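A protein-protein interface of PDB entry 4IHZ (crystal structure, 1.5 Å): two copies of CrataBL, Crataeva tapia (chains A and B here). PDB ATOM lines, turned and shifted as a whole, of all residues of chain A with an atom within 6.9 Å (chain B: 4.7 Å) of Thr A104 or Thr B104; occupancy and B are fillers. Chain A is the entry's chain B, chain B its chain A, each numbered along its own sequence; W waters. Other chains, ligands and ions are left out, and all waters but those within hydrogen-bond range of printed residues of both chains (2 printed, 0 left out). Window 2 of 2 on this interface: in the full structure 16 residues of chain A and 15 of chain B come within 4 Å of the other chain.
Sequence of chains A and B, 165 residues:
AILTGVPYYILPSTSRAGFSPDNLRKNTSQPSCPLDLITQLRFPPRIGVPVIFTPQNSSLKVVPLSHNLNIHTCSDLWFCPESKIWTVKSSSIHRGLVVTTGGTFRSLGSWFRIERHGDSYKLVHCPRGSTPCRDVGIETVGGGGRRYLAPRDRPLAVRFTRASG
The backbone carbonyl oxygen (O) of Ser B83 is in hydrogen-bond range of the backbone NH (N) of Gly B102.
OG of Ser B83 lies within hydrogen-bond range of O of Gly B103 (2.6 Å).
OG of Ser B107 is in hydrogen-bond range of O of Thr B104, 3.1 Å away.
OG of Ser A83 sits at hydrogen-bond distance from N of Ile A85, at 3.1 Å.
The backbone carbonyl oxygen (O) of Ser A83 lies within hydrogen-bond range of the backbone NH (N) of Gly A102.
The backbone carbonyl oxygen (O) of Gly A103 lies within hydrogen-bond range of the side-chain hydroxyl (OG) of Ser A83 (2.6 Å).
Among the printed residues, pairs that only touch across the chains: Thr A104 with Thr B104 (3.5 Å) and Ser A83 with Ser B83 (3.6 Å).
Printed residues of chain B within 4 Å of Thr A104: Thr B104.
Of the printed residues of chain A, Thr B104 touches Thr A104.
Of the printed residues of chain A, Ser B83 touches Ser A83 (3.6 Å).
Printed residues of chain B within 4 Å of Ser A83: Ser B83.
Arg A106 touches none of the printed residues of chain B.
The nearest printed residue of chain B that does not touch Thr A104 is Gly B103 (5.8 Å).
Of the 15 printed residues of chain A, 2 touch a printed residue of chain B.
Printed residues of chain A that touch a printed residue of chain B: Ser A83 and Thr A104.
Among the printed residues, no Asp or Glu carboxylate lies within 4 Å of a Lys or Arg side-chain nitrogen of the other chain.
Ser A83 touches its own counterpart, Ser B83.
Thr A104 touches its own counterpart, Thr B104.
Water W1 lies within hydrogen-bond range of the side-chain hydroxyl of Thr A104 and the side-chain hydroxyl of Thr B104.
Water W2 lies within hydrogen-bond range of OG1 of Thr B104, OG1 of Thr A104, O of Gly B103 and O of Gly A103.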
ATOM      1  N   ASN A  70       8.505  11.034 -29.882  1.00  0.00           N
ATOM      2  CA  ASN A  70       7.220  11.130 -29.217  1.00  0.00           C
ATOM      3  C   ASN A  70       6.858  12.588 -28.947  1.00  0.00           C
ATOM      4  O   ASN A  70       7.736  13.475 -28.831  1.00  0.00           O
ATOM      5  CB  ASN A  70       7.184  10.335 -27.892  1.00  0.00           C
ATOM      6  CG  ASN A  70       7.288   8.863 -28.111  1.00  0.00           C
ATOM      7  OD1 ASN A  70       7.776   8.158 -27.254  1.00  0.00           O
ATOM      8  ND2 ASN A  70       6.928   8.391 -29.315  1.00  0.00           N
ATOM      9  N   SER A  83      -2.877   8.893 -20.727  1.00  0.00           N
ATOM     10  CA  SER A  83      -1.659   9.751 -20.766  1.00  0.00           C
ATOM     11  C   SER A  83      -1.846  11.008 -21.610  1.00  0.00           C
ATOM     12  O   SER A  83      -2.842  11.174 -22.356  1.00  0.00           O
ATOM     13  CB  SER A  83      -0.511   8.937 -21.377  1.00  0.00           C
ATOM     14  OG  SER A  83      -0.707   8.926 -22.803  1.00  0.00           O
ATOM     15  N   ILE A  85       0.333  11.596 -23.933  1.00  0.00           N
ATOM     16  CA  ILE A  85       1.238  11.264 -25.030  1.00  0.00           C
ATOM     17  C   ILE A  85       0.427  11.124 -26.305  1.00  0.00           C
ATOM     18  O   ILE A  85      -0.619  10.470 -26.310  1.00  0.00           O
ATOM     19  CB  ILE A  85       2.035   9.999 -24.699  1.00  0.00           C
ATOM     20  CG1 ILE A  85       2.872  10.268 -23.437  1.00  0.00           C
ATOM     21  CG2 ILE A  85       2.917   9.523 -25.907  1.00  0.00           C
ATOM     22  CD1 ILE A  85       3.240   9.015 -22.682  1.00  0.00           C
ATOM     23  N   TRP A  86       0.899  11.736 -27.381  1.00  0.00           N
ATOM     24  CA  TRP A  86       0.137  11.690 -28.624  1.00  0.00           C
ATOM     25  C   TRP A  86       0.310  10.354 -29.322  1.00  0.00           C
ATOM     26  O   TRP A  86       1.365   9.699 -29.224  1.00  0.00           O
ATOM     27  CB  TRP A  86       0.608  12.825 -29.550  1.00  0.00           C
ATOM     28  CG  TRP A  86       0.222  14.193 -29.064  1.00  0.00           C
ATOM     29  CD1 TRP A  86      -0.004  14.600 -27.754  1.00  0.00           C
ATOM     30  CD2 TRP A  86       0.085  15.363 -29.873  1.00  0.00           C
ATOM     31  NE1 TRP A  86      -0.345  15.949 -27.731  1.00  0.00           N
ATOM     32  CE2 TRP A  86      -0.246  16.442 -29.008  1.00  0.00           C
ATOM     33  CE3 TRP A  86       0.223  15.604 -31.253  1.00  0.00           C
ATOM     34  CZ2 TRP A  86      -0.494  17.758 -29.495  1.00  0.00           C
ATOM     35  CZ3 TRP A  86       0.012  16.929 -31.728  1.00  0.00           C
ATOM     36  CH2 TRP A  86      -0.344  17.960 -30.851  1.00  0.00           C
ATOM     37  N   THR A  87      -0.761   9.968 -30.029  1.00  0.00           N
ATOM     38  CA  THR A  87      -0.815   8.730 -30.809  1.00  0.00           C
ATOM     39  C   THR A  87      -1.861   8.937 -31.913  1.00  0.00           C
ATOM     40  O   THR A  87      -2.361  10.058 -32.133  1.00  0.00           O
ATOM     41  CB  THR A  87      -1.158   7.518 -29.893  1.00  0.00           C
ATOM     42  OG1 THR A  87      -1.062   6.289 -30.635  1.00  0.00           O
ATOM     43  CG2 THR A  87      -2.543   7.680 -29.228  1.00  0.00           C
ATOM     44  N   GLY A 102      -3.326   9.982 -25.017  1.00  0.00           N
ATOM     45  CA  GLY A 102      -3.591   8.682 -24.429  1.00  0.00           C
ATOM     46  C   GLY A 102      -2.650   7.584 -24.909  1.00  0.00           C
ATOM     47  O   GLY A 102      -2.918   6.383 -24.652  1.00  0.00           O
ATOM     48  N   GLY A 103      -1.577   7.969 -25.606  1.00  0.00           N
ATOM     49  CA  GLY A 103      -0.571   7.041 -26.093  1.00  0.00           C
ATOM     50  C   GLY A 103       0.400   6.536 -25.036  1.00  0.00           C
ATOM     51  O   GLY A 103       0.268   6.776 -23.834  1.00  0.00           O
ATOM     52  N   THR A 104       1.393   5.830 -25.513  1.00  0.00           N
ATOM     53  CA  THR A 104       2.382   5.226 -24.628  1.00  0.00           C
ATOM     54  C   THR A 104       3.755   5.577 -25.170  1.00  0.00           C
ATOM     55  O   THR A 104       4.008   5.503 -26.369  1.00  0.00           O
ATOM     56  CB  THR A 104       2.155   3.686 -24.537  1.00  0.00           C
ATOM     57  OG1 THR A 104       0.894   3.443 -23.897  1.00  0.00           O
ATOM     58  CG2 THR A 104       3.246   3.055 -23.685  1.00  0.00           C
ATOM     59  N   PHE A 105       4.654   6.016 -24.287  1.00  0.00           N
ATOM     60  CA  PHE A 105       5.980   6.371 -24.744  1.00  0.00           C
ATOM     61  C   PHE A 105       6.652   5.169 -25.426  1.00  0.00           C
ATOM     62  O   PHE A 105       6.584   4.033 -24.913  1.00  0.00           O
ATOM     63  CB  PHE A 105       6.879   6.755 -23.572  1.00  0.00           C
ATOM     64  CG  PHE A 105       6.802   8.204 -23.162  1.00  0.00           C
ATOM     65  CD1 PHE A 105       6.815   9.231 -24.102  1.00  0.00           C
ATOM     66  CD2 PHE A 105       6.767   8.530 -21.816  1.00  0.00           C
ATOM     67  CE1 PHE A 105       6.793  10.561 -23.681  1.00  0.00           C
ATOM     68  CE2 PHE A 105       6.755   9.844 -21.387  1.00  0.00           C
ATOM     69  CZ  PHE A 105       6.776  10.852 -22.294  1.00  0.00           C
ATOM     70  N   ARG A 106       7.283   5.452 -26.569  1.00  0.00           N
ATOM     71  CA  ARG A 106       8.072   4.493 -27.344  1.00  0.00           C
ATOM     72  C   ARG A 106       7.259   3.315 -27.891  1.00  0.00           C
ATOM     73  O   ARG A 106       7.818   2.291 -28.325  1.00  0.00           O
ATOM     74  CB  ARG A 106       9.295   4.012 -26.532  1.00  0.00           C
ATOM     75  CG  ARG A 106      10.202   5.158 -25.975  1.00  0.00           C
ATOM     76  CD  ARG A 106      11.468   4.660 -25.238  1.00  0.00           C
ATOM     77  NE  ARG A 106      12.441   4.013 -26.128  1.00  0.00           N
ATOM     78  CZ  ARG A 106      13.312   4.628 -26.944  1.00  0.00           C
ATOM     79  NH1 ARG A 106      14.131   3.890 -27.686  1.00  0.00           N
ATOM     80  NH2 ARG A 106      13.390   5.957 -27.034  1.00  0.00           N
ATOM     81  N   SER A 107       5.948   3.430 -27.879  1.00  0.00           N
ATOM     82  CA  SER A 107       5.098   2.373 -28.421  1.00  0.00           C
ATOM     83  C   SER A 107       5.117   2.424 -29.948  1.00  0.00           C
ATOM     84  O   SER A 107       5.405   3.463 -30.553  1.00  0.00           O
ATOM     85  CB  SER A 107       3.659   2.482 -27.898  1.00  0.00           C
ATOM     86  OG  SER A 107       3.000   3.628 -28.409  1.00  0.00           O
ATOM     87  N   LEU A 108       4.790   1.291 -30.564  1.00  0.00           N
ATOM     88  CA  LEU A 108       4.750   1.212 -32.035  1.00  0.00           C
ATOM     89  C   LEU A 108       3.897   2.287 -32.734  1.00  0.00           C
ATOM     90  O   LEU A 108       4.218   2.678 -33.854  1.00  0.00           O
ATOM     91  CB  LEU A 108       4.256  -0.177 -32.448  1.00  0.00           C
ATOM     92  CG  LEU A 108       5.296  -1.289 -32.307  1.00  0.00           C
ATOM     93  CD1 LEU A 108       4.573  -2.625 -32.426  1.00  0.00           C
ATOM     94  CD2 LEU A 108       6.331  -1.145 -33.398  1.00  0.00           C
ATOM     95  N   GLY A 109       2.820   2.735 -32.087  1.00  0.00           N
ATOM     96  CA  GLY A 109       1.883   3.693 -32.677  1.00  0.00           C
ATOM     97  C   GLY A 109       2.084   5.144 -32.265  1.00  0.00           C
ATOM     98  O   GLY A 109       1.285   6.019 -32.656  1.00  0.00           O
ATOM     99  N   SER A 110       3.173   5.390 -31.544  1.00  0.00           N
ATOM    100  CA  SER A 110       3.483   6.676 -30.877  1.00  0.00           C
ATOM    101  C   SER A 110       4.400   7.587 -31.678  1.00  0.00           C
ATOM    102  O   SER A 110       4.710   8.668 -31.212  1.00  0.00           O
ATOM    103  CB  SER A 110       4.226   6.433 -29.513  1.00  0.00           C
ATOM    104  OG  SER A 110       5.622   5.964 -29.631  1.00  0.00           O
ATOM    105  N   TRP A 111       4.890   7.129 -32.832  1.00  0.00           N
ATOM    106  CA  TRP A 111       5.993   7.779 -33.506  1.00  0.00           C
ATOM    107  C   TRP A 111       5.541   8.826 -34.510  1.00  0.00           C
ATOM    108  O   TRP A 111       4.790   8.515 -35.452  1.00  0.00           O
ATOM    109  CB  TRP A 111       6.904   6.735 -34.167  1.00  0.00           C
ATOM    110  CG  TRP A 111       7.560   5.810 -33.196  1.00  0.00           C
ATOM    111  CD1 TRP A 111       7.368   4.468 -33.129  1.00  0.00           C
ATOM    112  CD2 TRP A 111       8.492   6.151 -32.154  1.00  0.00           C
ATOM    113  NE1 TRP A 111       8.167   3.928 -32.122  1.00  0.00           N
ATOM    114  CE2 TRP A 111       8.841   4.947 -31.496  1.00  0.00           C
ATOM    115  CE3 TRP A 111       9.078   7.358 -31.720  1.00  0.00           C
ATOM    116  CZ2 TRP A 111       9.754   4.912 -30.432  1.00  0.00           C
ATOM    117  CZ3 TRP A 111       9.975   7.331 -30.645  1.00  0.00           C
ATOM    118  CH2 TRP A 111      10.300   6.103 -30.011  1.00  0.00           C
ATOM    119  N   SER B  83       0.021   8.031 -17.902  1.00  0.00           N
ATOM    120  CA  SER B  83      -1.368   7.995 -17.450  1.00  0.00           C
ATOM    121  C   SER B  83      -1.483   7.986 -15.905  1.00  0.00           C
ATOM    122  O   SER B  83      -0.508   7.760 -15.184  1.00  0.00           O
ATOM    123  CB  SER B  83      -2.008   6.709 -17.946  1.00  0.00           C
ATOM    124  OG  SER B  83      -1.536   5.641 -17.128  1.00  0.00           O
ATOM    125  N   ILE B  85      -3.298   5.567 -14.635  1.00  0.00           N
ATOM    126  CA  ILE B  85      -3.807   4.209 -14.483  1.00  0.00           C
ATOM    127  C   ILE B  85      -2.756   3.362 -13.762  1.00  0.00           C
ATOM    128  O   ILE B  85      -1.582   3.401 -14.074  1.00  0.00           O
ATOM    129  CB  ILE B  85      -4.128   3.653 -15.867  1.00  0.00           C
ATOM    130  CG1 ILE B  85      -5.238   4.507 -16.513  1.00  0.00           C
ATOM    131  CG2 ILE B  85      -4.542   2.118 -15.783  1.00  0.00           C
ATOM    132  CD1 ILE B  85      -5.267   4.425 -18.026  1.00  0.00           C
ATOM    133  N   GLY B 102       0.861   5.137 -14.627  1.00  0.00           N
ATOM    134  CA  GLY B 102       1.474   5.128 -15.935  1.00  0.00           C
ATOM    135  C   GLY B 102       1.106   3.893 -16.750  1.00  0.00           C
ATOM    136  O   GLY B 102       1.714   3.646 -17.812  1.00  0.00           O
ATOM    137  N   GLY B 103       0.109   3.149 -16.291  1.00  0.00           N
ATOM    138  CA  GLY B 103      -0.405   1.985 -17.008  1.00  0.00           C
ATOM    139  C   GLY B 103      -1.310   2.319 -18.183  1.00  0.00           C
ATOM    140  O   GLY B 103      -1.462   3.470 -18.593  1.00  0.00           O
ATOM    141  N   THR B 104      -1.915   1.273 -18.740  1.00  0.00           N
ATOM    142  CA  THR B 104      -2.778   1.430 -19.920  1.00  0.00           C
ATOM    143  C   THR B 104      -4.073   0.669 -19.626  1.00  0.00           C
ATOM    144  O   THR B 104      -4.009  -0.467 -19.131  1.00  0.00           O
ATOM    145  CB  THR B 104      -2.045   0.891 -21.176  1.00  0.00           C
ATOM    146  OG1 THR B 104      -0.868   1.676 -21.395  1.00  0.00           O
ATOM    147  CG2 THR B 104      -2.916   1.038 -22.422  1.00  0.00           C
ATOM    148  N   PHE B 105      -5.239   1.279 -19.871  1.00  0.00           N
ATOM    149  CA  PHE B 105      -6.506   0.573 -19.620  1.00  0.00           C
ATOM    150  C   PHE B 105      -6.560  -0.752 -20.403  1.00  0.00           C
ATOM    151  O   PHE B 105      -6.222  -0.810 -21.601  1.00  0.00           O
ATOM    152  CB  PHE B 105      -7.726   1.395 -20.057  1.00  0.00           C
ATOM    153  CG  PHE B 105      -8.208   2.422 -19.052  1.00  0.00           C
ATOM    154  CD1 PHE B 105      -8.361   2.113 -17.705  1.00  0.00           C
ATOM    155  CD2 PHE B 105      -8.602   3.682 -19.505  1.00  0.00           C
ATOM    156  CE1 PHE B 105      -8.849   3.093 -16.811  1.00  0.00           C
ATOM    157  CE2 PHE B 105      -9.078   4.667 -18.644  1.00  0.00           C
ATOM    158  CZ  PHE B 105      -9.217   4.370 -17.285  1.00  0.00           C
ATOM    159  N   ARG B 106      -6.974  -1.801 -19.702  1.00  0.00           N
ATOM    160  CA  ARG B 106      -7.265  -3.114 -20.279  1.00  0.00           C
ATOM    161  C   ARG B 106      -6.027  -3.825 -20.806  1.00  0.00           C
ATOM    162  O   ARG B 106      -6.145  -4.853 -21.486  1.00  0.00           O
ATOM    163  CB  ARG B 106      -8.382  -3.047 -21.334  1.00  0.00           C
ATOM    164  CG  ARG B 106      -9.739  -2.610 -20.809  1.00  0.00           C
ATOM    165  CD  ARG B 106     -10.779  -2.430 -21.930  1.00  0.00           C
ATOM    166  NE  ARG B 106     -10.436  -1.279 -22.762  1.00  0.00           N
ATOM    167  CZ  ARG B 106     -10.673  -0.004 -22.434  1.00  0.00           C
ATOM    168  NH1 ARG B 106     -11.276   0.315 -21.288  1.00  0.00           N
ATOM    169  NH2 ARG B 106     -10.307   0.961 -23.264  1.00  0.00           N
ATOM    170  N   SER B 107      -4.841  -3.308 -20.478  1.00  0.00           N
ATOM    171  CA  SER B 107      -3.593  -3.955 -20.854  1.00  0.00           C
ATOM    172  C   SER B 107      -3.311  -5.166 -19.964  1.00  0.00           C
ATOM    173  O   SER B 107      -3.878  -5.329 -18.853  1.00  0.00           O
ATOM    174  CB  SER B 107      -2.415  -2.972 -20.861  1.00  0.00           C
ATOM    175  OG  SER B 107      -1.982  -2.736 -19.546  1.00  0.00           O
ATOM    176  N   SER B 110      -2.426  -4.446 -16.349  1.00  0.00           N
ATOM    177  CA  SER B 110      -3.309  -3.438 -15.713  1.00  0.00           C
ATOM    178  C   SER B 110      -4.275  -3.991 -14.672  1.00  0.00           C
ATOM    179  O   SER B 110      -5.004  -3.234 -14.035  1.00  0.00           O
ATOM    180  CB  SER B 110      -4.212  -2.756 -16.788  1.00  0.00           C
ATOM    181  OG  SER B 110      -5.217  -3.662 -17.326  1.00  0.00           O
HETATM  182  O   HOH W   1       0.367   0.588 -23.832  1.00  0.00           O
HETATM  183  O   HOH W   2      -0.622   4.648 -21.484  1.00  0.00           O
